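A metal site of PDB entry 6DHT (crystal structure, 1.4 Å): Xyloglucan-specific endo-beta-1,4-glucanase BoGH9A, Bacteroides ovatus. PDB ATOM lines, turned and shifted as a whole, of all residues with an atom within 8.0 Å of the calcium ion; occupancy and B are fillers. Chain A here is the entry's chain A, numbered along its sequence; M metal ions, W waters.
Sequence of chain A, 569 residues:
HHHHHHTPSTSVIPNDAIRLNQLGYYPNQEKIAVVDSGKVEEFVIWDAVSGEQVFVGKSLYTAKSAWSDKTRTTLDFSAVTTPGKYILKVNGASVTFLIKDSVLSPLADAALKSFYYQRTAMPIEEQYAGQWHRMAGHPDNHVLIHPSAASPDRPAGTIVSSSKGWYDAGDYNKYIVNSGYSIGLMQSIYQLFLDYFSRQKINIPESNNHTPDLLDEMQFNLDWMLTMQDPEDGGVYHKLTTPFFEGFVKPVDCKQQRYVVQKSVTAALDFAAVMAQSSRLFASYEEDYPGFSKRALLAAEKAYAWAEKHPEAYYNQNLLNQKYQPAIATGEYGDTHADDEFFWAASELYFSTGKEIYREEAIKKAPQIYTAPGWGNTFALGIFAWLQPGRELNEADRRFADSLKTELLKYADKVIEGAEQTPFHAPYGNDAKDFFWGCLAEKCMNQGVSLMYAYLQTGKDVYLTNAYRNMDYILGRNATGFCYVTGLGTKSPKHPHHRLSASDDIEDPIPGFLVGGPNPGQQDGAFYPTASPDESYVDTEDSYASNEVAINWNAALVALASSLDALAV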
ATOM      1  N   VAL A 177      -9.594 -13.373  -8.874  1.00  0.00           N
ATOM      2  CA  VAL A 177      -8.211 -13.751  -8.617  1.00  0.00           C
ATOM      3  C   VAL A 177      -7.868 -15.007  -9.396  1.00  0.00           C
ATOM      4  O   VAL A 177      -6.873 -15.046 -10.163  1.00  0.00           O
ATOM      5  CB  VAL A 177      -7.940 -13.908  -7.121  1.00  0.00           C
ATOM      6  CG1 VAL A 177      -6.649 -14.656  -6.846  1.00  0.00           C
ATOM      7  CG2 VAL A 177      -7.915 -12.537  -6.461  1.00  0.00           C
ATOM      8  N   THR A 266      -5.960  -7.664  -4.484  1.00  0.00           N
ATOM      9  CA  THR A 266      -5.476  -8.756  -5.341  1.00  0.00           C
ATOM     10  C   THR A 266      -6.381  -8.923  -6.573  1.00  0.00           C
ATOM     11  O   THR A 266      -5.906  -9.138  -7.677  1.00  0.00           O
ATOM     12  CB  THR A 266      -5.381 -10.048  -4.555  1.00  0.00           C
ATOM     13  OG1 THR A 266      -6.581 -10.214  -3.792  1.00  0.00           O
ATOM     14  CG2 THR A 266      -4.189  -9.991  -3.625  1.00  0.00           C
ATOM     15  N   ASP A 270      -4.718  -8.567 -10.205  1.00  0.00           N
ATOM     16  CA  ASP A 270      -4.757  -9.666 -11.168  1.00  0.00           C
ATOM     17  C   ASP A 270      -5.591  -9.260 -12.387  1.00  0.00           C
ATOM     18  O   ASP A 270      -5.253  -9.567 -13.528  1.00  0.00           O
ATOM     19  CB  ASP A 270      -5.344 -10.907 -10.536  1.00  0.00           C
ATOM     20  CG  ASP A 270      -4.406 -11.546  -9.525  1.00  0.00           C
ATOM     21  OD1 ASP A 270      -3.183 -11.331  -9.626  1.00  0.00           O
ATOM     22  OD2 ASP A 270      -4.887 -12.252  -8.598  1.00  0.00           O
ATOM     23  N   GLY A 334      -8.020 -15.890  -0.406  1.00  0.00           N
ATOM     24  CA  GLY A 334      -7.501 -14.832   0.447  1.00  0.00           C
ATOM     25  C   GLY A 334      -5.999 -14.765   0.385  1.00  0.00           C
ATOM     26  O   GLY A 334      -5.332 -15.765   0.060  1.00  0.00           O
ATOM     27  N   ASP A 335      -5.456 -13.594   0.697  1.00  0.00           N
ATOM     28  CA  ASP A 335      -4.029 -13.352   0.555  1.00  0.00           C
ATOM     29  C   ASP A 335      -3.702 -12.029   1.244  1.00  0.00           C
ATOM     30  O   ASP A 335      -4.380 -11.031   0.997  1.00  0.00           O
ATOM     31  CB  ASP A 335      -3.702 -13.252  -0.948  1.00  0.00           C
ATOM     32  CG  ASP A 335      -2.213 -13.296  -1.269  1.00  0.00           C
ATOM     33  OD1 ASP A 335      -1.359 -13.504  -0.380  1.00  0.00           O
ATOM     34  OD2 ASP A 335      -1.904 -13.176  -2.482  1.00  0.00           O
ATOM     35  N   THR A 336      -2.693 -12.036   2.103  1.00  0.00           N
ATOM     36  CA  THR A 336      -2.235 -10.791   2.740  1.00  0.00           C
ATOM     37  C   THR A 336      -0.877 -10.325   2.206  1.00  0.00           C
ATOM     38  O   THR A 336      -0.261  -9.410   2.755  1.00  0.00           O
ATOM     39  CB  THR A 336      -2.136 -10.934   4.276  1.00  0.00           C
ATOM     40  OG1 THR A 336      -1.255 -12.018   4.605  1.00  0.00           O
ATOM     41  CG2 THR A 336      -3.496 -11.181   4.862  1.00  0.00           C
ATOM     42  N   HIS A 337      -0.440 -10.946   1.106  1.00  0.00           N
ATOM     43  CA  HIS A 337       0.837 -10.620   0.478  1.00  0.00           C
ATOM     44  C   HIS A 337       0.589 -10.258  -0.975  1.00  0.00           C
ATOM     45  O   HIS A 337       0.499 -11.141  -1.836  1.00  0.00           O
ATOM     46  CB  HIS A 337       1.822 -11.781   0.593  1.00  0.00           C
ATOM     47  CG  HIS A 337       2.216 -12.123   1.992  1.00  0.00           C
ATOM     48  ND1 HIS A 337       1.525 -13.038   2.761  1.00  0.00           N
ATOM     49  CD2 HIS A 337       3.233 -11.683   2.762  1.00  0.00           C
ATOM     50  CE1 HIS A 337       2.099 -13.134   3.944  1.00  0.00           C
ATOM     51  NE2 HIS A 337       3.141 -12.324   3.976  1.00  0.00           N
ATOM     52  N   ALA A 338       0.497  -8.967  -1.251  1.00  0.00           N
ATOM     53  CA  ALA A 338       0.157  -8.473  -2.578  1.00  0.00           C
ATOM     54  C   ALA A 338       1.374  -8.012  -3.405  1.00  0.00           C
ATOM     55  O   ALA A 338       1.216  -7.514  -4.524  1.00  0.00           O
ATOM     56  CB  ALA A 338      -0.851  -7.335  -2.459  1.00  0.00           C
ATOM     57  N   ASP A 339       2.583  -8.164  -2.867  1.00  0.00           N
ATOM     58  CA  ASP A 339       3.770  -7.689  -3.595  1.00  0.00           C
ATOM     59  C   ASP A 339       3.878  -8.347  -4.962  1.00  0.00           C
ATOM     60  O   ASP A 339       4.221  -7.682  -5.956  1.00  0.00           O
ATOM     61  CB  ASP A 339       5.058  -7.961  -2.822  1.00  0.00           C
ATOM     62  CG  ASP A 339       5.296  -6.968  -1.678  1.00  0.00           C
ATOM     63  OD1 ASP A 339       4.540  -5.987  -1.547  1.00  0.00           O
ATOM     64  OD2 ASP A 339       6.271  -7.174  -0.913  1.00  0.00           O
ATOM     65  N   ASP A 340       3.594  -9.647  -5.015  1.00  0.00           N
ATOM     66  CA  ASP A 340       3.746 -10.394  -6.268  1.00  0.00           C
ATOM     67  C   ASP A 340       2.723  -9.978  -7.327  1.00  0.00           C
ATOM     68  O   ASP A 340       3.035  -9.919  -8.525  1.00  0.00           O
ATOM     69  CB  ASP A 340       3.694 -11.904  -6.039  1.00  0.00           C
ATOM     70  CG  ASP A 340       2.509 -12.346  -5.191  1.00  0.00           C
ATOM     71  OD1 ASP A 340       2.489 -12.061  -3.974  1.00  0.00           O
ATOM     72  OD2 ASP A 340       1.587 -13.015  -5.725  1.00  0.00           O
ATOM     73  N   GLU A 341       1.508  -9.644  -6.893  1.00  0.00           N
ATOM     74  CA  GLU A 341       0.483  -9.153  -7.799  1.00  0.00           C
ATOM     75  C   GLU A 341       0.868  -7.728  -8.281  1.00  0.00           C
ATOM     76  O   GLU A 341       0.653  -7.393  -9.437  1.00  0.00           O
ATOM     77  CB  GLU A 341      -0.901  -9.176  -7.125  1.00  0.00           C
ATOM     78  CG  GLU A 341      -1.503 -10.595  -6.920  1.00  0.00           C
ATOM     79  CD  GLU A 341      -0.980 -11.329  -5.706  1.00  0.00           C
ATOM     80  OE1 GLU A 341      -0.194 -10.747  -4.920  1.00  0.00           O
ATOM     81  OE2 GLU A 341      -1.356 -12.506  -5.498  1.00  0.00           O
ATOM     82  N   PHE A 342       1.404  -6.904  -7.388  1.00  0.00           N
ATOM     83  CA  PHE A 342       1.920  -5.596  -7.808  1.00  0.00           C
ATOM     84  C   PHE A 342       3.038  -5.791  -8.844  1.00  0.00           C
ATOM     85  O   PHE A 342       3.054  -5.117  -9.872  1.00  0.00           O
ATOM     86  CB  PHE A 342       2.419  -4.787  -6.595  1.00  0.00           C
ATOM     87  CG  PHE A 342       1.360  -3.947  -5.923  1.00  0.00           C
ATOM     88  CD1 PHE A 342       0.825  -2.852  -6.579  1.00  0.00           C
ATOM     89  CD2 PHE A 342       0.915  -4.251  -4.659  1.00  0.00           C
ATOM     90  CE1 PHE A 342      -0.139  -2.068  -5.986  1.00  0.00           C
ATOM     91  CE2 PHE A 342      -0.058  -3.460  -4.044  1.00  0.00           C
ATOM     92  CZ  PHE A 342      -0.580  -2.362  -4.729  1.00  0.00           C
ATOM     93  N   GLY A 374       1.384 -19.779  -9.031  1.00  0.00           N
ATOM     94  CA  GLY A 374       0.159 -20.236  -8.387  1.00  0.00           C
ATOM     95  C   GLY A 374      -0.782 -19.068  -8.242  1.00  0.00           C
ATOM     96  O   GLY A 374      -0.372 -17.921  -8.344  1.00  0.00           O
ATOM     97  N   TRP A 375      -2.053 -19.357  -7.983  1.00  0.00           N
ATOM     98  CA  TRP A 375      -3.058 -18.293  -7.990  1.00  0.00           C
ATOM     99  C   TRP A 375      -2.738 -17.124  -7.057  1.00  0.00           C
ATOM    100  O   TRP A 375      -3.058 -15.993  -7.359  1.00  0.00           O
ATOM    101  CB  TRP A 375      -4.470 -18.831  -7.743  1.00  0.00           C
ATOM    102  CG  TRP A 375      -4.728 -19.445  -6.384  1.00  0.00           C
ATOM    103  CD1 TRP A 375      -4.751 -20.768  -6.097  1.00  0.00           C
ATOM    104  CD2 TRP A 375      -4.997 -18.752  -5.141  1.00  0.00           C
ATOM    105  NE1 TRP A 375      -5.043 -20.955  -4.748  1.00  0.00           N
ATOM    106  CE2 TRP A 375      -5.192 -19.728  -4.158  1.00  0.00           C
ATOM    107  CE3 TRP A 375      -5.101 -17.402  -4.796  1.00  0.00           C
ATOM    108  CZ2 TRP A 375      -5.487 -19.396  -2.821  1.00  0.00           C
ATOM    109  CZ3 TRP A 375      -5.393 -17.079  -3.459  1.00  0.00           C
ATOM    110  CH2 TRP A 375      -5.570 -18.072  -2.504  1.00  0.00           C
ATOM    111  N   GLY A 376      -2.087 -17.417  -5.935  1.00  0.00           N
ATOM    112  CA  GLY A 376      -1.778 -16.407  -4.941  1.00  0.00           C
ATOM    113  C   GLY A 376      -0.335 -15.950  -4.975  1.00  0.00           C
ATOM    114  O   GLY A 376       0.080 -15.100  -4.185  1.00  0.00           O
ATOM    115  N   ASN A 377       0.437 -16.513  -5.894  1.00  0.00           N
ATOM    116  CA  ASN A 377       1.845 -16.204  -6.037  1.00  0.00           C
ATOM    117  C   ASN A 377       2.180 -15.997  -7.508  1.00  0.00           C
ATOM    118  O   ASN A 377       2.577 -16.925  -8.225  1.00  0.00           O
ATOM    119  CB  ASN A 377       2.739 -17.301  -5.467  1.00  0.00           C
ATOM    120  CG  ASN A 377       4.243 -16.975  -5.656  1.00  0.00           C
ATOM    121  OD1 ASN A 377       4.649 -15.845  -6.054  1.00  0.00           O
ATOM    122  ND2 ASN A 377       5.082 -17.967  -5.384  1.00  0.00           N
ATOM    123  N   THR A 378       2.034 -14.745  -7.923  1.00  0.00           N
ATOM    124  CA  THR A 378       2.100 -14.416  -9.348  1.00  0.00           C
ATOM    125  C   THR A 378       3.476 -13.871  -9.750  1.00  0.00           C
ATOM    126  O   THR A 378       3.627 -13.346 -10.857  1.00  0.00           O
ATOM    127  CB  THR A 378       1.012 -13.414  -9.733  1.00  0.00           C
ATOM    128  OG1 THR A 378       1.163 -12.192  -8.981  1.00  0.00           O
ATOM    129  CG2 THR A 378      -0.364 -13.972  -9.430  1.00  0.00           C
ATOM    130  N   PHE A 379       4.477 -14.005  -8.889  1.00  0.00           N
ATOM    131  CA  PHE A 379       5.832 -13.539  -9.274  1.00  0.00           C
ATOM    132  C   PHE A 379       6.241 -14.140 -10.601  1.00  0.00           C
ATOM    133  O   PHE A 379       6.770 -13.440 -11.473  1.00  0.00           O
ATOM    134  CB  PHE A 379       6.879 -13.886  -8.217  1.00  0.00           C
ATOM    135  CG  PHE A 379       7.010 -12.882  -7.085  1.00  0.00           C
ATOM    136  CD1 PHE A 379       7.096 -11.519  -7.332  1.00  0.00           C
ATOM    137  CD2 PHE A 379       7.126 -13.316  -5.782  1.00  0.00           C
ATOM    138  CE1 PHE A 379       7.263 -10.621  -6.289  1.00  0.00           C
ATOM    139  CE2 PHE A 379       7.269 -12.415  -4.746  1.00  0.00           C
ATOM    140  CZ  PHE A 379       7.343 -11.066  -5.021  1.00  0.00           C
HETATM  141 CA    CA M   1       0.202 -12.817  -3.571  1.00  0.00          CA
HETATM  142  O   HOH W   1       1.068 -14.128  -1.666  1.00  0.00           O
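Within 4 Å of the calcium ion: Asp 335, His 337, Asp 340, Glu 341 and Gly 376. The nearest printed residue that does not touch the calcium ion is Asn 377 (4.4 Å).
O of Asp 340 is in hydrogen-bond range of OG1 of Thr 378, at 3.0 Å. The side-chain hydroxyl (OG1) of Thr 336 sits at hydrogen-bond distance from a ring nitrogen (ND1) of His 337, at 3.5 Å. N of Glu 341 lies within hydrogen-bond range of OG1 of Thr 378, at 3.3 Å.
The calcium ion is bound by O of Gly 376 (2.4 Å), OD2 of Asp 335 (2.4 Å), O of His 337 (2.4 Å), OD1 of Asp 340 (2.4 Å), water W1 (2.5 Å), OE2 of Glu 341 (2.5 Å), OE1 of Glu 341 (2.5 Å) and OD2 of Asp 340 (2.6 Å). The calcium ion has eight donor atoms within binding distance.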
